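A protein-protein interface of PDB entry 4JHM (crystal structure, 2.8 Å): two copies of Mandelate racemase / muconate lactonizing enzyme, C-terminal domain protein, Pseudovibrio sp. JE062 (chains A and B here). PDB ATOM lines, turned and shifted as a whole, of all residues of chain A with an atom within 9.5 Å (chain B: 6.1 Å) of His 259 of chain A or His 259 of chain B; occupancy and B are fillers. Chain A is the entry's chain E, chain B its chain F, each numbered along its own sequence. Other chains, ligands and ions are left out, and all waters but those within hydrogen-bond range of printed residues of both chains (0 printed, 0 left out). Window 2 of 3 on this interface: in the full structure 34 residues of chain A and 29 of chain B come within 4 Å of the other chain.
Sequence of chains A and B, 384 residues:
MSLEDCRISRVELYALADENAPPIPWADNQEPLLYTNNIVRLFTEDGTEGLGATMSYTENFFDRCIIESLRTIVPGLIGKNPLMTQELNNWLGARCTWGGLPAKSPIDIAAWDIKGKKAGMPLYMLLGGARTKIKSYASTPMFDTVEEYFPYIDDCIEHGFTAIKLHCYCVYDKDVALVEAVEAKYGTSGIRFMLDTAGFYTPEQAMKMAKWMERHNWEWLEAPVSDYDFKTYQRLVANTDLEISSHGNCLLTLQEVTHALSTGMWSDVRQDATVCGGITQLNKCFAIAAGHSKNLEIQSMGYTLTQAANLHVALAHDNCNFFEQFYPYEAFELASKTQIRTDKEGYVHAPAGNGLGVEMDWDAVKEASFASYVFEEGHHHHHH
CB of Gln 255 of chain B touches O of Tyr 228 of chain A, 3.1 Å away.
Tyr 228 of chain A touches Glu 256 of chain B.
Asp 229 of chain A touches Gln 255 of chain B.
His 259 of chain B touches Phe 230 of chain A (CD2 to CD2, 3.6 Å).
His 259 of chain A touches Phe 230 of chain B.
His 259 of chain A touches His 259 of chain B.
The backbone carbonyl oxygen of His 259 of chain A sits at hydrogen-bond distance from the side-chain hydroxyl of Thr 263 of chain A.
The backbone carbonyl oxygen of His 259 of chain B sits at hydrogen-bond distance from the side-chain hydroxyl of Thr 263 of chain B.
Phe 230 of chain A touches His 259 of chain B, and with the chains exchanged His 259 of chain A touches Phe 230 of chain B.
His 259 of chain A touches its own counterpart, His 259 of chain B.
Positions printed for both chains: 230, 254, 255, 256, 257, 258, 259, 260, 261, 262, 263, 264 and 265.
Of the printed residues of chain B, Tyr 228 of chain A touches Gln 255 (3.1 Å) and Glu 256 (3.3 Å).
Of the printed residues of chain B, Phe 230 of chain A touches His 259 (3.6 Å).
Leu 251 of chain A touches none of the printed residues of chain B.
His 259 of chain A touches just these residues of chain B: Phe 230 and His 259.
Of the printed residues of chain A, Phe 230 of chain B touches His 259.
No residue of chain A comes within 4 Å of Thr 258 of chain B.
His 259 of chain B touches just these residues of chain A: Phe 230 and His 259.
Ala 260 of chain B touches none of the printed residues of chain A.
No residue of chain A comes within 4 Å of Ser 262 of chain B.
The nearest residue of chain B that does not touch His 259 of chain A is Met 265 of chain B (5.0 Å).
The nearest residue of chain A that does not touch His 259 of chain B is Met 265 of chain A (5.1 Å).
The nearest printed residue of chain B that does not touch Phe 230 of chain A is Glu 256 of chain B (4.9 Å).
Of the 23 printed residues of chain A, 4 touch a printed residue of chain B.
Printed residues of chain B that touch a printed residue of chain A: Phe 230, Gln 255, Glu 256 and His 259.
Hydrophobic or aromatic side chains of chain B that line the printed part of chain A: Phe 230 and His 259.
Along chain B the printed residues that touch a printed residue of chain A span positions 230 to 259.
Among the printed residues, no Asp or Glu carboxylate lies within 4 Å of a Lys or Arg side-chain nitrogen of the other chain.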
ATOM      1  N   ASP A 227      17.181  -5.590 -26.601  1.00  0.00           N
ATOM      2  CA  ASP A 227      18.616  -5.589 -26.341  1.00  0.00           C
ATOM      3  C   ASP A 227      19.341  -6.610 -27.215  1.00  0.00           C
ATOM      4  O   ASP A 227      20.563  -6.575 -27.331  1.00  0.00           O
ATOM      5  CB  ASP A 227      18.909  -5.865 -24.864  1.00  0.00           C
ATOM      6  CG  ASP A 227      18.780  -4.625 -24.002  1.00  0.00           C
ATOM      7  OD1 ASP A 227      17.902  -3.784 -24.291  1.00  0.00           O
ATOM      8  OD2 ASP A 227      19.553  -4.490 -23.031  1.00  0.00           O
ATOM      9  N   TYR A 228      18.587  -7.510 -27.835  1.00  0.00           N
ATOM     10  CA  TYR A 228      19.184  -8.575 -28.628  1.00  0.00           C
ATOM     11  C   TYR A 228      19.269  -8.222 -30.109  1.00  0.00           C
ATOM     12  O   TYR A 228      19.984  -8.872 -30.867  1.00  0.00           O
ATOM     13  CB  TYR A 228      18.434  -9.887 -28.401  1.00  0.00           C
ATOM     14  CG  TYR A 228      18.572 -10.354 -26.971  1.00  0.00           C
ATOM     15  CD1 TYR A 228      19.796 -10.810 -26.487  1.00  0.00           C
ATOM     16  CD2 TYR A 228      17.494 -10.308 -26.090  1.00  0.00           C
ATOM     17  CE1 TYR A 228      19.937 -11.224 -25.176  1.00  0.00           C
ATOM     18  CE2 TYR A 228      17.629 -10.719 -24.776  1.00  0.00           C
ATOM     19  CZ  TYR A 228      18.852 -11.172 -24.328  1.00  0.00           C
ATOM     20  OH  TYR A 228      18.995 -11.579 -23.030  1.00  0.00           O
ATOM     21  N   ASP A 229      18.553  -7.181 -30.514  1.00  0.00           N
ATOM     22  CA  ASP A 229      18.688  -6.649 -31.862  1.00  0.00           C
ATOM     23  C   ASP A 229      19.975  -5.832 -31.888  1.00  0.00           C
ATOM     24  O   ASP A 229      19.959  -4.620 -31.679  1.00  0.00           O
ATOM     25  CB  ASP A 229      17.473  -5.790 -32.219  1.00  0.00           C
ATOM     26  CG  ASP A 229      17.545  -5.208 -33.626  1.00  0.00           C
ATOM     27  OD1 ASP A 229      18.466  -5.574 -34.394  1.00  0.00           O
ATOM     28  OD2 ASP A 229      16.673  -4.375 -33.958  1.00  0.00           O
ATOM     29  N   PHE A 230      21.095  -6.509 -32.116  1.00  0.00           N
ATOM     30  CA  PHE A 230      22.396  -5.857 -32.050  1.00  0.00           C
ATOM     31  C   PHE A 230      22.529  -4.809 -33.142  1.00  0.00           C
ATOM     32  O   PHE A 230      22.930  -3.677 -32.884  1.00  0.00           O
ATOM     33  CB  PHE A 230      23.539  -6.874 -32.188  1.00  0.00           C
ATOM     34  CG  PHE A 230      23.599  -7.891 -31.083  1.00  0.00           C
ATOM     35  CD1 PHE A 230      23.079  -7.622 -29.827  1.00  0.00           C
ATOM     36  CD2 PHE A 230      24.207  -9.119 -31.297  1.00  0.00           C
ATOM     37  CE1 PHE A 230      23.146  -8.563 -28.817  1.00  0.00           C
ATOM     38  CE2 PHE A 230      24.283 -10.062 -30.289  1.00  0.00           C
ATOM     39  CZ  PHE A 230      23.751  -9.784 -29.047  1.00  0.00           C
ATOM     40  N   LYS A 231      22.186  -5.190 -34.365  1.00  0.00           N
ATOM     41  CA  LYS A 231      22.425  -4.327 -35.514  1.00  0.00           C
ATOM     42  C   LYS A 231      21.748  -2.962 -35.386  1.00  0.00           C
ATOM     43  O   LYS A 231      22.348  -1.938 -35.729  1.00  0.00           O
ATOM     44  CB  LYS A 231      21.996  -5.023 -36.799  1.00  0.00           C
ATOM     45  CG  LYS A 231      22.915  -6.162 -37.191  1.00  0.00           C
ATOM     46  CD  LYS A 231      22.622  -6.639 -38.600  1.00  0.00           C
ATOM     47  CE  LYS A 231      23.800  -7.400 -39.177  1.00  0.00           C
ATOM     48  NZ  LYS A 231      23.667  -7.542 -40.652  1.00  0.00           N
ATOM     49  N   GLN A 234      23.858  -0.921 -33.036  1.00  0.00           N
ATOM     50  CA  GLN A 234      25.014  -0.495 -33.814  1.00  0.00           C
ATOM     51  C   GLN A 234      24.661   0.682 -34.728  1.00  0.00           C
ATOM     52  O   GLN A 234      25.389   1.674 -34.793  1.00  0.00           O
ATOM     53  CB  GLN A 234      25.548  -1.662 -34.643  1.00  0.00           C
ATOM     54  CG  GLN A 234      26.056  -2.823 -33.804  1.00  0.00           C
ATOM     55  CD  GLN A 234      26.611  -3.953 -34.647  1.00  0.00           C
ATOM     56  OE1 GLN A 234      25.944  -4.460 -35.552  1.00  0.00           O
ATOM     57  NE2 GLN A 234      27.837  -4.360 -34.349  1.00  0.00           N
ATOM     58  N   LEU A 251      21.763  -8.361 -21.061  1.00  0.00           N
ATOM     59  CA  LEU A 251      23.160  -8.745 -21.252  1.00  0.00           C
ATOM     60  C   LEU A 251      23.934  -8.473 -19.966  1.00  0.00           C
ATOM     61  O   LEU A 251      24.343  -7.341 -19.702  1.00  0.00           O
ATOM     62  CB  LEU A 251      23.769  -7.991 -22.431  1.00  0.00           C
ATOM     63  CG  LEU A 251      23.470  -8.594 -23.810  1.00  0.00           C
ATOM     64  CD1 LEU A 251      22.004  -8.945 -23.960  1.00  0.00           C
ATOM     65  CD2 LEU A 251      23.890  -7.647 -24.915  1.00  0.00           C
ATOM     66  N   THR A 253      26.488 -10.768 -18.539  1.00  0.00           N
ATOM     67  CA  THR A 253      27.798 -11.393 -18.412  1.00  0.00           C
ATOM     68  C   THR A 253      28.897 -10.395 -18.749  1.00  0.00           C
ATOM     69  O   THR A 253      28.712  -9.526 -19.606  1.00  0.00           O
ATOM     70  CB  THR A 253      27.948 -12.609 -19.353  1.00  0.00           C
ATOM     71  OG1 THR A 253      27.929 -12.169 -20.717  1.00  0.00           O
ATOM     72  CG2 THR A 253      26.831 -13.617 -19.124  1.00  0.00           C
ATOM     73  N   LEU A 254      30.040 -10.530 -18.079  1.00  0.00           N
ATOM     74  CA  LEU A 254      31.215  -9.719 -18.398  1.00  0.00           C
ATOM     75  C   LEU A 254      31.577  -9.822 -19.876  1.00  0.00           C
ATOM     76  O   LEU A 254      32.037  -8.850 -20.472  1.00  0.00           O
ATOM     77  CB  LEU A 254      32.416 -10.152 -17.560  1.00  0.00           C
ATOM     78  CG  LEU A 254      32.299  -9.960 -16.051  1.00  0.00           C
ATOM     79  CD1 LEU A 254      33.552 -10.472 -15.366  1.00  0.00           C
ATOM     80  CD2 LEU A 254      32.066  -8.500 -15.719  1.00  0.00           C
ATOM     81  N   GLN A 255      31.364 -10.995 -20.466  1.00  0.00           N
ATOM     82  CA  GLN A 255      31.695 -11.208 -21.873  1.00  0.00           C
ATOM     83  C   GLN A 255      30.710 -10.509 -22.795  1.00  0.00           C
ATOM     84  O   GLN A 255      31.091 -10.036 -23.858  1.00  0.00           O
ATOM     85  CB  GLN A 255      31.743 -12.700 -22.215  1.00  0.00           C
ATOM     86  CG  GLN A 255      32.799 -13.481 -21.448  1.00  0.00           C
ATOM     87  CD  GLN A 255      32.268 -14.080 -20.163  1.00  0.00           C
ATOM     88  OE1 GLN A 255      31.582 -13.414 -19.389  1.00  0.00           O
ATOM     89  NE2 GLN A 255      32.576 -15.349 -19.935  1.00  0.00           N
ATOM     90  N   GLU A 256      29.447 -10.444 -22.398  1.00  0.00           N
ATOM     91  CA  GLU A 256      28.448  -9.788 -23.235  1.00  0.00           C
ATOM     92  C   GLU A 256      28.647  -8.281 -23.227  1.00  0.00           C
ATOM     93  O   GLU A 256      28.484  -7.620 -24.255  1.00  0.00           O
ATOM     94  CB  GLU A 256      27.034 -10.135 -22.782  1.00  0.00           C
ATOM     95  CG  GLU A 256      26.542 -11.455 -23.336  1.00  0.00           C
ATOM     96  CD  GLU A 256      25.232 -11.871 -22.723  1.00  0.00           C
ATOM     97  OE1 GLU A 256      25.162 -11.917 -21.478  1.00  0.00           O
ATOM     98  OE2 GLU A 256      24.279 -12.150 -23.486  1.00  0.00           O
ATOM     99  N   VAL A 257      28.995  -7.747 -22.063  1.00  0.00           N
ATOM    100  CA  VAL A 257      29.339  -6.346 -21.953  1.00  0.00           C
ATOM    101  C   VAL A 257      30.516  -6.061 -22.880  1.00  0.00           C
ATOM    102  O   VAL A 257      30.472  -5.136 -23.692  1.00  0.00           O
ATOM    103  CB  VAL A 257      29.736  -5.978 -20.511  1.00  0.00           C
ATOM    104  CG1 VAL A 257      30.372  -4.595 -20.466  1.00  0.00           C
ATOM    105  CG2 VAL A 257      28.522  -6.044 -19.596  1.00  0.00           C
ATOM    106  N   THR A 258      31.562  -6.874 -22.758  1.00  0.00           N
ATOM    107  CA  THR A 258      32.789  -6.672 -23.525  1.00  0.00           C
ATOM    108  C   THR A 258      32.521  -6.751 -25.021  1.00  0.00           C
ATOM    109  O   THR A 258      33.035  -5.953 -25.799  1.00  0.00           O
ATOM    110  CB  THR A 258      33.854  -7.712 -23.154  1.00  0.00           C
ATOM    111  OG1 THR A 258      34.113  -7.645 -21.750  1.00  0.00           O
ATOM    112  CG2 THR A 258      35.132  -7.447 -23.898  1.00  0.00           C
ATOM    113  N   HIS A 259      31.711  -7.717 -25.425  1.00  0.00           N
ATOM    114  CA  HIS A 259      31.377  -7.860 -26.830  1.00  0.00           C
ATOM    115  C   HIS A 259      30.659  -6.614 -27.340  1.00  0.00           C
ATOM    116  O   HIS A 259      31.011  -6.070 -28.382  1.00  0.00           O
ATOM    117  CB  HIS A 259      30.503  -9.094 -27.044  1.00  0.00           C
ATOM    118  CG  HIS A 259      30.137  -9.322 -28.474  1.00  0.00           C
ATOM    119  ND1 HIS A 259      28.911  -8.964 -28.993  1.00  0.00           N
ATOM    120  CD2 HIS A 259      30.845  -9.846 -29.501  1.00  0.00           C
ATOM    121  CE1 HIS A 259      28.875  -9.271 -30.277  1.00  0.00           C
ATOM    122  NE2 HIS A 259      30.037  -9.804 -30.612  1.00  0.00           N
ATOM    123  N   ALA A 260      29.657  -6.161 -26.596  1.00  0.00           N
ATOM    124  CA  ALA A 260      28.831  -5.047 -27.036  1.00  0.00           C
ATOM    125  C   ALA A 260      29.670  -3.792 -27.239  1.00  0.00           C
ATOM    126  O   ALA A 260      29.569  -3.117 -28.267  1.00  0.00           O
ATOM    127  CB  ALA A 260      27.726  -4.787 -26.030  1.00  0.00           C
ATOM    128  N   LEU A 261      30.504  -3.480 -26.257  1.00  0.00           N
ATOM    129  CA  LEU A 261      31.339  -2.298 -26.338  1.00  0.00           C
ATOM    130  C   LEU A 261      32.345  -2.411 -27.483  1.00  0.00           C
ATOM    131  O   LEU A 261      32.722  -1.407 -28.086  1.00  0.00           O
ATOM    132  CB  LEU A 261      32.047  -2.059 -25.007  1.00  0.00           C
ATOM    133  CG  LEU A 261      31.137  -1.460 -23.934  1.00  0.00           C
ATOM    134  CD1 LEU A 261      31.909  -1.216 -22.650  1.00  0.00           C
ATOM    135  CD2 LEU A 261      30.510  -0.163 -24.411  1.00  0.00           C
ATOM    136  N   SER A 262      32.757  -3.638 -27.788  1.00  0.00           N
ATOM    137  CA  SER A 262      33.705  -3.896 -28.868  1.00  0.00           C
ATOM    138  C   SER A 262      33.078  -3.808 -30.255  1.00  0.00           C
ATOM    139  O   SER A 262      33.786  -3.595 -31.237  1.00  0.00           O
ATOM    140  CB  SER A 262      34.338  -5.282 -28.704  1.00  0.00           C
ATOM    141  OG  SER A 262      35.239  -5.303 -27.614  1.00  0.00           O
ATOM    142  N   THR A 263      31.762  -3.979 -30.342  1.00  0.00           N
ATOM    143  CA  THR A 263      31.071  -3.984 -31.640  1.00  0.00           C
ATOM    144  C   THR A 263      30.257  -2.707 -31.889  1.00  0.00           C
ATOM    145  O   THR A 263      29.511  -2.619 -32.867  1.00  0.00           O
ATOM    146  CB  THR A 263      30.131  -5.194 -31.757  1.00  0.00           C
ATOM    147  OG1 THR A 263      29.295  -5.262 -30.599  1.00  0.00           O
ATOM    148  CG2 THR A 263      30.925  -6.471 -31.855  1.00  0.00           C
ATOM    149  N   GLY A 264      30.394  -1.731 -30.997  1.00  0.00           N
ATOM    150  CA  GLY A 264      29.787  -0.423 -31.191  1.00  0.00           C
ATOM    151  C   GLY A 264      28.310  -0.365 -30.856  1.00  0.00           C
ATOM    152  O   GLY A 264      27.622   0.562 -31.273  1.00  0.00           O
ATOM    153  N   MET A 265      27.827  -1.344 -30.093  1.00  0.00           N
ATOM    154  CA  MET A 265      26.404  -1.434 -29.752  1.00  0.00           C
ATOM    155  C   MET A 265      25.907  -0.387 -28.793  1.00  0.00           C
ATOM    156  O   MET A 265      24.782   0.081 -28.935  1.00  0.00           O
ATOM    157  CB  MET A 265      26.112  -2.766 -29.080  1.00  0.00           C
ATOM    158  CG  MET A 265      25.908  -3.863 -30.111  1.00  0.00           C
ATOM    159  SD  MET A 265      25.774  -5.585 -29.171  1.00  0.00           S
ATOM    160  CE  MET A 265      26.675  -6.650 -30.562  1.00  0.00           C
ATOM    161  N   TRP A 266      26.717  -0.032 -27.797  1.00  0.00           N
ATOM    162  CA  TRP A 266      26.286   0.880 -26.732  1.00  0.00           C
ATOM    163  C   TRP A 266      27.206   2.085 -26.602  1.00  0.00           C
ATOM    164  O   TRP A 266      28.424   1.957 -26.734  1.00  0.00           O
ATOM    165  CB  TRP A 266      26.284   0.183 -25.367  1.00  0.00           C
ATOM    166  CG  TRP A 266      25.498  -1.102 -25.250  1.00  0.00           C
ATOM    167  CD1 TRP A 266      24.442  -1.500 -26.012  1.00  0.00           C
ATOM    168  CD2 TRP A 266      25.692  -2.128 -24.268  1.00  0.00           C
ATOM    169  NE1 TRP A 266      23.980  -2.723 -25.578  1.00  0.00           N
ATOM    170  CE2 TRP A 266      24.730  -3.125 -24.505  1.00  0.00           C
ATOM    171  CE3 TRP A 266      26.594  -2.298 -23.210  1.00  0.00           C
ATOM    172  CZ2 TRP A 266      24.642  -4.275 -23.731  1.00  0.00           C
ATOM    173  CZ3 TRP A 266      26.504  -3.438 -22.439  1.00  0.00           C
ATOM    174  CH2 TRP A 266      25.534  -4.414 -22.704  1.00  0.00           C
ATOM    175  N   ILE A 288      35.942  -2.615 -17.227  1.00  0.00           N
ATOM    176  CA  ILE A 288      35.780  -2.942 -18.643  1.00  0.00           C
ATOM    177  C   ILE A 288      35.360  -1.705 -19.432  1.00  0.00           C
ATOM    178  O   ILE A 288      35.880  -1.439 -20.516  1.00  0.00           O
ATOM    179  CB  ILE A 288      34.725  -4.048 -18.847  1.00  0.00           C
ATOM    180  CG1 ILE A 288      35.263  -5.394 -18.357  1.00  0.00           C
ATOM    181  CG2 ILE A 288      34.334  -4.146 -20.313  1.00  0.00           C
ATOM    182  CD1 ILE A 288      34.237  -6.509 -18.373  1.00  0.00           C
ATOM    183  N   HIS A 292      37.152   0.887 -22.455  1.00  0.00           N
ATOM    184  CA  HIS A 292      36.532   1.273 -23.712  1.00  0.00           C
ATOM    185  C   HIS A 292      36.269   2.783 -23.771  1.00  0.00           C
ATOM    186  O   HIS A 292      35.602   3.271 -24.685  1.00  0.00           O
ATOM    187  CB  HIS A 292      35.234   0.498 -23.910  1.00  0.00           C
ATOM    188  CG  HIS A 292      35.442  -0.910 -24.367  1.00  0.00           C
ATOM    189  ND1 HIS A 292      35.761  -1.227 -25.669  1.00  0.00           N
ATOM    190  CD2 HIS A 292      35.365  -2.086 -23.702  1.00  0.00           C
ATOM    191  CE1 HIS A 292      35.878  -2.538 -25.785  1.00  0.00           C
ATOM    192  NE2 HIS A 292      35.648  -3.082 -24.605  1.00  0.00           N
ATOM    193  N   PHE B 230      32.341 -15.902 -27.065  1.00  0.00           N
ATOM    194  CA  PHE B 230      32.044 -16.035 -28.483  1.00  0.00           C
ATOM    195  C   PHE B 230      33.276 -16.372 -29.308  1.00  0.00           C
ATOM    196  O   PHE B 230      33.199 -17.144 -30.259  1.00  0.00           O
ATOM    197  CB  PHE B 230      31.425 -14.742 -29.019  1.00  0.00           C
ATOM    198  CG  PHE B 230      30.065 -14.436 -28.460  1.00  0.00           C
ATOM    199  CD1 PHE B 230      29.257 -15.443 -27.955  1.00  0.00           C
ATOM    200  CD2 PHE B 230      29.579 -13.135 -28.472  1.00  0.00           C
ATOM    201  CE1 PHE B 230      28.001 -15.155 -27.451  1.00  0.00           C
ATOM    202  CE2 PHE B 230      28.321 -12.841 -27.973  1.00  0.00           C
ATOM    203  CZ  PHE B 230      27.531 -13.853 -27.459  1.00  0.00           C
ATOM    204  N   LEU B 254      15.690 -15.354 -30.781  1.00  0.00           N
ATOM    205  CA  LEU B 254      15.884 -15.543 -32.215  1.00  0.00           C
ATOM    206  C   LEU B 254      17.067 -14.714 -32.702  1.00  0.00           C
ATOM    207  O   LEU B 254      17.855 -15.173 -33.535  1.00  0.00           O
ATOM    208  CB  LEU B 254      14.616 -15.153 -32.981  1.00  0.00           C
ATOM    209  CG  LEU B 254      13.344 -15.929 -32.626  1.00  0.00           C
ATOM    210  CD1 LEU B 254      12.144 -15.293 -33.301  1.00  0.00           C
ATOM    211  CD2 LEU B 254      13.459 -17.390 -33.019  1.00  0.00           C
ATOM    212  N   GLN B 255      17.190 -13.498 -32.169  1.00  0.00           N
ATOM    213  CA  GLN B 255      18.297 -12.598 -32.505  1.00  0.00           C
ATOM    214  C   GLN B 255      19.655 -13.209 -32.160  1.00  0.00           C
ATOM    215  O   GLN B 255      20.578 -13.188 -32.971  1.00  0.00           O
ATOM    216  CB  GLN B 255      18.139 -11.257 -31.778  1.00  0.00           C
ATOM    217  CG  GLN B 255      16.974 -10.404 -32.266  1.00  0.00           C
ATOM    218  CD  GLN B 255      15.617 -10.982 -31.898  1.00  0.00           C
ATOM    219  OE1 GLN B 255      14.933 -11.561 -32.738  1.00  0.00           O
ATOM    220  NE2 GLN B 255      15.227 -10.838 -30.634  1.00  0.00           N
ATOM    221  N   GLU B 256      19.776 -13.756 -30.956  1.00  0.00           N
ATOM    222  CA  GLU B 256      21.030 -14.362 -30.531  1.00  0.00           C
ATOM    223  C   GLU B 256      21.396 -15.546 -31.406  1.00  0.00           C
ATOM    224  O   GLU B 256      22.571 -15.782 -31.678  1.00  0.00           O
ATOM    225  CB  GLU B 256      20.945 -14.818 -29.083  1.00  0.00           C
ATOM    226  CG  GLU B 256      20.910 -13.685 -28.085  1.00  0.00           C
ATOM    227  CD  GLU B 256      20.674 -14.178 -26.679  1.00  0.00           C
ATOM    228  OE1 GLU B 256      19.572 -14.702 -26.401  1.00  0.00           O
ATOM    229  OE2 GLU B 256      21.598 -14.040 -25.855  1.00  0.00           O
ATOM    230  N   VAL B 257      20.388 -16.294 -31.839  1.00  0.00           N
ATOM    231  CA  VAL B 257      20.624 -17.461 -32.683  1.00  0.00           C
ATOM    232  C   VAL B 257      21.080 -16.997 -34.066  1.00  0.00           C
ATOM    233  O   VAL B 257      22.047 -17.524 -34.628  1.00  0.00           O
ATOM    234  CB  VAL B 257      19.367 -18.354 -32.771  1.00  0.00           C
ATOM    235  CG1 VAL B 257      19.457 -19.316 -33.948  1.00  0.00           C
ATOM    236  CG2 VAL B 257      19.176 -19.118 -31.465  1.00  0.00           C
ATOM    237  N   THR B 258      20.389 -15.989 -34.587  1.00  0.00           N
ATOM    238  CA  THR B 258      20.728 -15.392 -35.872  1.00  0.00           C
ATOM    239  C   THR B 258      22.172 -14.893 -35.885  1.00  0.00           C
ATOM    240  O   THR B 258      22.871 -15.009 -36.897  1.00  0.00           O
ATOM    241  CB  THR B 258      19.803 -14.200 -36.180  1.00  0.00           C
ATOM    242  OG1 THR B 258      18.438 -14.636 -36.215  1.00  0.00           O
ATOM    243  CG2 THR B 258      20.167 -13.575 -37.513  1.00  0.00           C
ATOM    244  N   HIS B 259      22.611 -14.339 -34.757  1.00  0.00           N
ATOM    245  CA  HIS B 259      23.926 -13.709 -34.659  1.00  0.00           C
ATOM    246  C   HIS B 259      25.029 -14.751 -34.591  1.00  0.00           C
ATOM    247  O   HIS B 259      26.075 -14.616 -35.235  1.00  0.00           O
ATOM    248  CB  HIS B 259      23.983 -12.817 -33.417  1.00  0.00           C
ATOM    249  CG  HIS B 259      25.321 -12.191 -33.182  1.00  0.00           C
ATOM    250  ND1 HIS B 259      26.212 -12.669 -32.247  1.00  0.00           N
ATOM    251  CD2 HIS B 259      25.920 -11.125 -33.759  1.00  0.00           C
ATOM    252  CE1 HIS B 259      27.304 -11.926 -32.259  1.00  0.00           C
ATOM    253  NE2 HIS B 259      27.154 -10.983 -33.168  1.00  0.00           N
ATOM    254  N   ALA B 260      24.783 -15.793 -33.801  1.00  0.00           N
ATOM    255  CA  ALA B 260      25.772 -16.837 -33.564  1.00  0.00           C
ATOM    256  C   ALA B 260      26.119 -17.531 -34.867  1.00  0.00           C
ATOM    257  O   ALA B 260      27.289 -17.765 -35.160  1.00  0.00           O
ATOM    258  CB  ALA B 260      25.245 -17.842 -32.549  1.00  0.00           C
ATOM    259  N   LEU B 261      25.097 -17.849 -35.654  1.00  0.00           N
ATOM    260  CA  LEU B 261      25.307 -18.494 -36.942  1.00  0.00           C
ATOM    261  C   LEU B 261      25.939 -17.521 -37.924  1.00  0.00           C
ATOM    262  O   LEU B 261      26.795 -17.899 -38.716  1.00  0.00           O
ATOM    263  CB  LEU B 261      23.986 -19.011 -37.491  1.00  0.00           C
ATOM    264  CG  LEU B 261      23.371 -20.119 -36.644  1.00  0.00           C
ATOM    265  CD1 LEU B 261      21.886 -20.246 -36.917  1.00  0.00           C
ATOM    266  CD2 LEU B 261      24.080 -21.430 -36.917  1.00  0.00           C
ATOM    267  N   SER B 262      25.523 -16.262 -37.860  1.00  0.00           N
ATOM    268  CA  SER B 262      26.085 -15.234 -38.731  1.00  0.00           C
ATOM    269  C   SER B 262      27.577 -15.037 -38.513  1.00  0.00           C
ATOM    270  O   SER B 262      28.301 -14.764 -39.462  1.00  0.00           O
ATOM    271  CB  SER B 262      25.370 -13.903 -38.532  1.00  0.00           C
ATOM    272  OG  SER B 262      24.054 -13.980 -39.035  1.00  0.00           O
ATOM    273  N   THR B 263      28.035 -15.166 -37.272  1.00  0.00           N
ATOM    274  CA  THR B 263      29.437 -14.902 -36.962  1.00  0.00           C
ATOM    275  C   THR B 263      30.203 -16.193 -36.707  1.00  0.00           C
ATOM    276  O   THR B 263      31.284 -16.179 -36.133  1.00  0.00           O
ATOM    277  CB  THR B 263      29.584 -13.962 -35.750  1.00  0.00           C
ATOM    278  OG1 THR B 263      29.043 -14.583 -34.586  1.00  0.00           O
ATOM    279  CG2 THR B 263      28.858 -12.654 -35.991  1.00  0.00           C
ATOM    280  N   GLY B 264      29.626 -17.309 -37.131  1.00  0.00           N
ATOM    281  CA  GLY B 264      30.326 -18.589 -37.125  1.00  0.00           C
ATOM    282  C   GLY B 264      30.745 -19.086 -35.762  1.00  0.00           C
ATOM    283  O   GLY B 264      31.882 -19.515 -35.583  1.00  0.00           O
ATOM    284  N   MET B 265      29.821 -19.046 -34.805  1.00  0.00           N
ATOM    285  CA  MET B 265      30.077 -19.545 -33.453  1.00  0.00           C
ATOM    286  C   MET B 265      29.708 -20.995 -33.309  1.00  0.00           C
ATOM    287  O   MET B 265      30.315 -21.717 -32.510  1.00  0.00           O
ATOM    288  CB  MET B 265      29.233 -18.788 -32.436  1.00  0.00           C
ATOM    289  CG  MET B 265      29.460 -17.287 -32.520  1.00  0.00           C
ATOM    290  SD  MET B 265      28.482 -16.421 -31.049  1.00  0.00           S
ATOM    291  CE  MET B 265      29.038 -14.598 -31.529  1.00  0.00           C
